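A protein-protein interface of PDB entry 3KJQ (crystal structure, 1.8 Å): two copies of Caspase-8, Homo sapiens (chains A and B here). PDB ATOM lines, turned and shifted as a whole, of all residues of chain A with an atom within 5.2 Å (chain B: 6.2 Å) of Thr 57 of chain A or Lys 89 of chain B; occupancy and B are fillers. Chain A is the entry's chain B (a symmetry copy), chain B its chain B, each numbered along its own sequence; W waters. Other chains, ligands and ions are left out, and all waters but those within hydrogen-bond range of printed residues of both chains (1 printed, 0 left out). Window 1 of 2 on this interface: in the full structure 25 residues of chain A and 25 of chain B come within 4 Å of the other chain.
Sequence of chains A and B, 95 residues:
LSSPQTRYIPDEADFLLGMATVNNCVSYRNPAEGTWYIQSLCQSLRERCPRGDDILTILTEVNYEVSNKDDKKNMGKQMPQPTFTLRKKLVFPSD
The side-chain amino group (NZ) of Lys 89 of chain B is in hydrogen-bond range of the side-chain hydroxyl (OG1) of Thr 57 of chain A.
The side-chain carboxylate (OD1) of Asp 54 of chain B is in salt-bridge range of the side-chain amino group (NZ) of Lys 89 of chain B, 3.8 Å away. The side-chain carboxylate (OD1) of Asp 54 of chain A lies within hydrogen-bond range of the side-chain hydroxyl (OG1) of Thr 57 of chain A (2.6 Å). The backbone carbonyl oxygen (O) of Leu 56 of chain A lies within hydrogen-bond range of the side-chain hydroxyl (OG1) of Thr 60 of chain A (2.9 Å). The side-chain carboxylate of Asp 54 of chain B lies within hydrogen-bond range of the backbone NH of Leu 56 of chain B (3.1 Å).
Among the printed residues, merely in contact across the chains: Thr 60 of chain A with Leu 56 of chain B (3.6 Å), Thr 60 of chain A with Leu 86 of chain B (3.9 Å), Thr 60 of chain A with Arg 87 of chain B (3.5 Å) and Thr 60 of chain A with Lys 88 of chain B (3.5 Å).
Of chain B, only Lys 89 comes within 4 Å of Thr 57 of chain A. Printed residues of chain A within 4 Å of Leu 86 of chain B: Thr 60 (3.9 Å). Printed residues of chain A within 4 Å of Arg 87 of chain B: Thr 60 (3.5 Å). Printed residues of chain A within 4 Å of Lys 88 of chain B: Thr 60. Val 91 of chain B touches none of the printed residues of chain A. The nearest residue of chain A that does not touch Lys 89 of chain B is Thr 60 of chain A (4.1 Å). The nearest printed residue of chain A that does not touch Lys 88 of chain B is Glu 61 of chain A (6.3 Å).
Of the 10 printed residues of chain A, 2 touch a printed residue of chain B. Hydrophobic or aromatic side chains of chain B within 4 Å of the printed part of chain A: Leu 56. Among the printed residues, 5 pairs touch across the chains.
Positions printed for both chains: 54, 55, 56 and 57.
Water W1 lies within hydrogen-bond range of O of Lys 88 of chain B (2.8 Å) and OG1 of Thr 60 of chain A (2.9 Å).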
ATOM      1  N   ARG A  48     -15.428   3.505  29.982  1.00  0.00           N
ATOM      2  CA  ARG A  48     -15.394   2.513  28.898  1.00  0.00           C
ATOM      3  C   ARG A  48     -16.752   2.137  28.306  1.00  0.00           C
ATOM      4  O   ARG A  48     -16.817   1.732  27.149  1.00  0.00           O
ATOM      5  CB  ARG A  48     -14.675   1.242  29.368  1.00  0.00           C
ATOM      6  CG  ARG A  48     -13.183   1.448  29.611  1.00  0.00           C
ATOM      7  CD  ARG A  48     -12.513   0.199  30.135  1.00  0.00           C
ATOM      8  NE  ARG A  48     -11.058   0.262  29.977  1.00  0.00           N
ATOM      9  CZ  ARG A  48     -10.353  -0.376  29.035  1.00  0.00           C
ATOM     10  NH1 ARG A  48      -9.031  -0.235  29.006  1.00  0.00           N
ATOM     11  NH2 ARG A  48     -10.943  -1.127  28.109  1.00  0.00           N
ATOM     12  N   ASP A  53     -17.189  -0.884  25.250  1.00  0.00           N
ATOM     13  CA  ASP A  53     -16.412  -1.996  25.812  1.00  0.00           C
ATOM     14  C   ASP A  53     -17.329  -2.902  26.628  1.00  0.00           C
ATOM     15  O   ASP A  53     -18.288  -2.433  27.245  1.00  0.00           O
ATOM     16  CB  ASP A  53     -15.279  -1.485  26.698  1.00  0.00           C
ATOM     17  CG  ASP A  53     -14.113  -0.886  25.904  1.00  0.00           C
ATOM     18  OD1 ASP A  53     -14.023  -1.108  24.678  1.00  0.00           O
ATOM     19  OD2 ASP A  53     -13.287  -0.173  26.513  1.00  0.00           O
ATOM     20  N   ASP A  54     -17.029  -4.198  26.640  1.00  0.00           N
ATOM     21  CA  ASP A  54     -17.859  -5.155  27.362  1.00  0.00           C
ATOM     22  C   ASP A  54     -17.396  -5.299  28.806  1.00  0.00           C
ATOM     23  O   ASP A  54     -16.297  -4.883  29.167  1.00  0.00           O
ATOM     24  CB  ASP A  54     -17.837  -6.524  26.686  1.00  0.00           C
ATOM     25  CG  ASP A  54     -16.487  -7.196  26.801  1.00  0.00           C
ATOM     26  OD1 ASP A  54     -15.540  -6.763  26.115  1.00  0.00           O
ATOM     27  OD2 ASP A  54     -16.373  -8.147  27.570  1.00  0.00           O
ATOM     28  N   ILE A  55     -18.237  -5.910  29.623  1.00  0.00           N
ATOM     29  CA  ILE A  55     -18.001  -5.965  31.061  1.00  0.00           C
ATOM     30  C   ILE A  55     -16.762  -6.788  31.428  1.00  0.00           C
ATOM     31  O   ILE A  55     -16.128  -6.501  32.443  1.00  0.00           O
ATOM     32  CB  ILE A  55     -19.236  -6.525  31.808  1.00  0.00           C
ATOM     33  CG1 ILE A  55     -19.169  -6.207  33.304  1.00  0.00           C
ATOM     34  CG2 ILE A  55     -19.373  -8.044  31.581  1.00  0.00           C
ATOM     35  CD1 ILE A  55     -19.065  -4.746  33.633  1.00  0.00           C
ATOM     36  N   LEU A  56     -16.420  -7.797  30.629  1.00  0.00           N
ATOM     37  CA  LEU A  56     -15.223  -8.615  30.928  1.00  0.00           C
ATOM     38  C   LEU A  56     -13.947  -7.825  30.661  1.00  0.00           C
ATOM     39  O   LEU A  56     -12.983  -7.928  31.430  1.00  0.00           O
ATOM     40  CB  LEU A  56     -15.219  -9.967  30.191  1.00  0.00           C
ATOM     41  CG  LEU A  56     -16.416 -10.891  30.501  1.00  0.00           C
ATOM     42  CD1 LEU A  56     -16.357 -12.206  29.694  1.00  0.00           C
ATOM     43  CD2 LEU A  56     -16.515 -11.189  31.996  1.00  0.00           C
ATOM     44  N   THR A  57     -13.943  -7.025  29.596  1.00  0.00           N
ATOM     45  CA  THR A  57     -12.821  -6.127  29.320  1.00  0.00           C
ATOM     46  C   THR A  57     -12.684  -5.120  30.472  1.00  0.00           C
ATOM     47  O   THR A  57     -11.587  -4.868  30.992  1.00  0.00           O
ATOM     48  CB  THR A  57     -13.013  -5.379  27.991  1.00  0.00           C
ATOM     49  OG1 THR A  57     -13.094  -6.315  26.913  1.00  0.00           O
ATOM     50  CG2 THR A  57     -11.851  -4.441  27.747  1.00  0.00           C
ATOM     51  N   ILE A  58     -13.818  -4.580  30.894  1.00  0.00           N
ATOM     52  CA  ILE A  58     -13.855  -3.626  31.999  1.00  0.00           C
ATOM     53  C   ILE A  58     -13.360  -4.251  33.314  1.00  0.00           C
ATOM     54  O   ILE A  58     -12.530  -3.666  34.015  1.00  0.00           O
ATOM     55  CB  ILE A  58     -15.278  -2.998  32.119  1.00  0.00           C
ATOM     56  CG1 ILE A  58     -15.503  -2.038  30.943  1.00  0.00           C
ATOM     57  CG2 ILE A  58     -15.465  -2.304  33.488  1.00  0.00           C
ATOM     58  CD1 ILE A  58     -16.951  -1.631  30.722  1.00  0.00           C
ATOM     59  N   LEU A  59     -13.818  -5.457  33.636  1.00  0.00           N
ATOM     60  CA  LEU A  59     -13.367  -6.111  34.866  1.00  0.00           C
ATOM     61  C   LEU A  59     -11.888  -6.532  34.820  1.00  0.00           C
ATOM     62  O   LEU A  59     -11.237  -6.635  35.858  1.00  0.00           O
ATOM     63  CB  LEU A  59     -14.256  -7.302  35.220  1.00  0.00           C
ATOM     64  CG  LEU A  59     -15.673  -6.934  35.672  1.00  0.00           C
ATOM     65  CD1 LEU A  59     -16.559  -8.188  35.728  1.00  0.00           C
ATOM     66  CD2 LEU A  59     -15.633  -6.222  37.042  1.00  0.00           C
ATOM     67  N   THR A  60     -11.370  -6.776  33.622  1.00  0.00           N
ATOM     68  CA  THR A  60      -9.936  -7.007  33.440  1.00  0.00           C
ATOM     69  C   THR A  60      -9.165  -5.742  33.838  1.00  0.00           C
ATOM     70  O   THR A  60      -8.182  -5.816  34.567  1.00  0.00           O
ATOM     71  CB  THR A  60      -9.607  -7.473  32.001  1.00  0.00           C
ATOM     72  OG1 THR A  60     -10.206  -8.763  31.756  1.00  0.00           O
ATOM     73  CG2 THR A  60      -8.097  -7.589  31.795  1.00  0.00           C
ATOM     74  N   GLU A  61      -9.638  -4.584  33.388  1.00  0.00           N
ATOM     75  CA  GLU A  61      -9.040  -3.308  33.782  1.00  0.00           C
ATOM     76  C   GLU A  61      -9.122  -3.066  35.292  1.00  0.00           C
ATOM     77  O   GLU A  61      -8.156  -2.583  35.892  1.00  0.00           O
ATOM     78  CB  GLU A  61      -9.675  -2.139  33.034  1.00  0.00           C
ATOM     79  CG  GLU A  61      -9.089  -0.805  33.452  1.00  0.00           C
ATOM     80  CD  GLU A  61      -9.496   0.309  32.537  1.00  0.00           C
ATOM     81  OE1 GLU A  61      -8.686   0.677  31.667  1.00  0.00           O
ATOM     82  OE2 GLU A  61     -10.621   0.815  32.675  1.00  0.00           O
ATOM     83  N   ASP B  54      -9.629 -12.506  22.147  1.00  0.00           N
ATOM     84  CA  ASP B  54      -9.023 -12.834  23.431  1.00  0.00           C
ATOM     85  C   ASP B  54      -9.718 -14.026  24.075  1.00  0.00           C
ATOM     86  O   ASP B  54     -10.813 -14.417  23.674  1.00  0.00           O
ATOM     87  CB  ASP B  54      -9.075 -11.644  24.386  1.00  0.00           C
ATOM     88  CG  ASP B  54     -10.488 -11.326  24.826  1.00  0.00           C
ATOM     89  OD1 ASP B  54     -11.266 -10.798  24.009  1.00  0.00           O
ATOM     90  OD2 ASP B  54     -10.816 -11.604  25.976  1.00  0.00           O
ATOM     91  N   ILE B  55      -9.081 -14.588  25.088  1.00  0.00           N
ATOM     92  CA  ILE B  55      -9.544 -15.835  25.685  1.00  0.00           C
ATOM     93  C   ILE B  55     -10.901 -15.692  26.380  1.00  0.00           C
ATOM     94  O   ILE B  55     -11.654 -16.664  26.436  1.00  0.00           O
ATOM     95  CB  ILE B  55      -8.504 -16.394  26.686  1.00  0.00           C
ATOM     96  CG1 ILE B  55      -8.771 -17.869  26.997  1.00  0.00           C
ATOM     97  CG2 ILE B  55      -8.486 -15.560  27.983  1.00  0.00           C
ATOM     98  CD1 ILE B  55      -8.779 -18.774  25.799  1.00  0.00           C
ATOM     99  N   LEU B  56     -11.214 -14.511  26.911  1.00  0.00           N
ATOM    100  CA  LEU B  56     -12.519 -14.314  27.582  1.00  0.00           C
ATOM    101  C   LEU B  56     -13.651 -14.280  26.562  1.00  0.00           C
ATOM    102  O   LEU B  56     -14.729 -14.832  26.816  1.00  0.00           O
ATOM    103  CB  LEU B  56     -12.543 -13.077  28.498  1.00  0.00           C
ATOM    104  CG  LEU B  56     -11.508 -13.084  29.644  1.00  0.00           C
ATOM    105  CD1 LEU B  56     -11.572 -11.795  30.491  1.00  0.00           C
ATOM    106  CD2 LEU B  56     -11.674 -14.314  30.534  1.00  0.00           C
ATOM    107  N   THR B  57     -13.408 -13.660  25.408  1.00  0.00           N
ATOM    108  CA  THR B  57     -14.377 -13.680  24.312  1.00  0.00           C
ATOM    109  C   THR B  57     -14.591 -15.129  23.853  1.00  0.00           C
ATOM    110  O   THR B  57     -15.725 -15.594  23.665  1.00  0.00           O
ATOM    111  CB  THR B  57     -13.905 -12.819  23.129  1.00  0.00           C
ATOM    112  OG1 THR B  57     -13.750 -11.460  23.546  1.00  0.00           O
ATOM    113  CG2 THR B  57     -14.914 -12.880  22.003  1.00  0.00           C
ATOM    114  N   LEU B  86      -6.858 -12.389  35.683  1.00  0.00           N
ATOM    115  CA  LEU B  86      -6.137 -11.747  34.588  1.00  0.00           C
ATOM    116  C   LEU B  86      -6.233 -10.231  34.673  1.00  0.00           C
ATOM    117  O   LEU B  86      -7.301  -9.679  34.956  1.00  0.00           O
ATOM    118  CB  LEU B  86      -6.669 -12.202  33.219  1.00  0.00           C
ATOM    119  CG  LEU B  86      -6.636 -13.693  32.894  1.00  0.00           C
ATOM    120  CD1 LEU B  86      -7.213 -13.940  31.486  1.00  0.00           C
ATOM    121  CD2 LEU B  86      -5.212 -14.280  33.035  1.00  0.00           C
ATOM    122  N   ARG B  87      -5.106  -9.571  34.409  1.00  0.00           N
ATOM    123  CA  ARG B  87      -5.009  -8.113  34.479  1.00  0.00           C
ATOM    124  C   ARG B  87      -4.869  -7.461  33.104  1.00  0.00           C
ATOM    125  O   ARG B  87      -4.877  -6.222  32.990  1.00  0.00           O
ATOM    126  CB  ARG B  87      -3.804  -7.715  35.336  1.00  0.00           C
ATOM    127  CG  ARG B  87      -3.867  -8.098  36.807  1.00  0.00           C
ATOM    128  CD  ARG B  87      -2.545  -7.820  37.519  1.00  0.00           C
ATOM    129  NE  ARG B  87      -1.433  -8.457  36.828  1.00  0.00           N
ATOM    130  CZ  ARG B  87      -0.487  -7.828  36.129  1.00  0.00           C
ATOM    131  NH1 ARG B  87      -0.416  -6.498  36.044  1.00  0.00           N
ATOM    132  NH2 ARG B  87       0.433  -8.538  35.521  1.00  0.00           N
ATOM    133  N   LYS B  88      -4.722  -8.285  32.073  1.00  0.00           N
ATOM    134  CA  LYS B  88      -4.594  -7.837  30.694  1.00  0.00           C
ATOM    135  C   LYS B  88      -5.388  -8.790  29.807  1.00  0.00           C
ATOM    136  O   LYS B  88      -5.799  -9.874  30.244  1.00  0.00           O
ATOM    137  CB  LYS B  88      -3.127  -7.833  30.244  1.00  0.00           C
ATOM    138  CG  LYS B  88      -2.156  -7.094  31.168  1.00  0.00           C
ATOM    139  CD  LYS B  88      -0.691  -7.248  30.738  1.00  0.00           C
ATOM    140  CE  LYS B  88       0.245  -6.434  31.630  1.00  0.00           C
ATOM    141  NZ  LYS B  88       1.665  -6.499  31.146  1.00  0.00           N
ATOM    142  N   LYS B  89      -5.614  -8.365  28.569  1.00  0.00           N
ATOM    143  CA  LYS B  89      -6.168  -9.230  27.536  1.00  0.00           C
ATOM    144  C   LYS B  89      -5.209 -10.395  27.276  1.00  0.00           C
ATOM    145  O   LYS B  89      -4.001 -10.193  27.167  1.00  0.00           O
ATOM    146  CB  LYS B  89      -6.344  -8.443  26.240  1.00  0.00           C
ATOM    147  CG  LYS B  89      -7.425  -7.368  26.301  1.00  0.00           C
ATOM    148  CD  LYS B  89      -8.766  -7.895  25.873  1.00  0.00           C
ATOM    149  CE  LYS B  89      -9.841  -6.810  25.937  1.00  0.00           C
ATOM    150  NZ  LYS B  89     -11.091  -7.265  25.265  1.00  0.00           N
ATOM    151  N   LEU B  90      -5.757 -11.598  27.166  1.00  0.00           N
ATOM    152  CA  LEU B  90      -4.974 -12.780  26.838  1.00  0.00           C
ATOM    153  C   LEU B  90      -5.282 -13.230  25.418  1.00  0.00           C
ATOM    154  O   LEU B  90      -6.383 -13.729  25.130  1.00  0.00           O
ATOM    155  CB  LEU B  90      -5.254 -13.910  27.825  1.00  0.00           C
ATOM    156  CG  LEU B  90      -4.505 -15.225  27.596  1.00  0.00           C
ATOM    157  CD1 LEU B  90      -2.987 -15.008  27.533  1.00  0.00           C
ATOM    158  CD2 LEU B  90      -4.863 -16.242  28.691  1.00  0.00           C
ATOM    159  N   VAL B  91      -4.302 -13.053  24.539  1.00  0.00           N
ATOM    160  CA  VAL B  91      -4.406 -13.496  23.144  1.00  0.00           C
ATOM    161  C   VAL B  91      -3.291 -14.498  22.851  1.00  0.00           C
ATOM    162  O   VAL B  91      -2.225 -14.427  23.454  1.00  0.00           O
ATOM    163  CB  VAL B  91      -4.324 -12.322  22.153  1.00  0.00           C
ATOM    164  CG1 VAL B  91      -5.529 -11.401  22.326  1.00  0.00           C
ATOM    165  CG2 VAL B  91      -2.993 -11.560  22.304  1.00  0.00           C
HETATM  166  O   HOH W   1      -8.537 -10.624  30.271  1.00  0.00           O
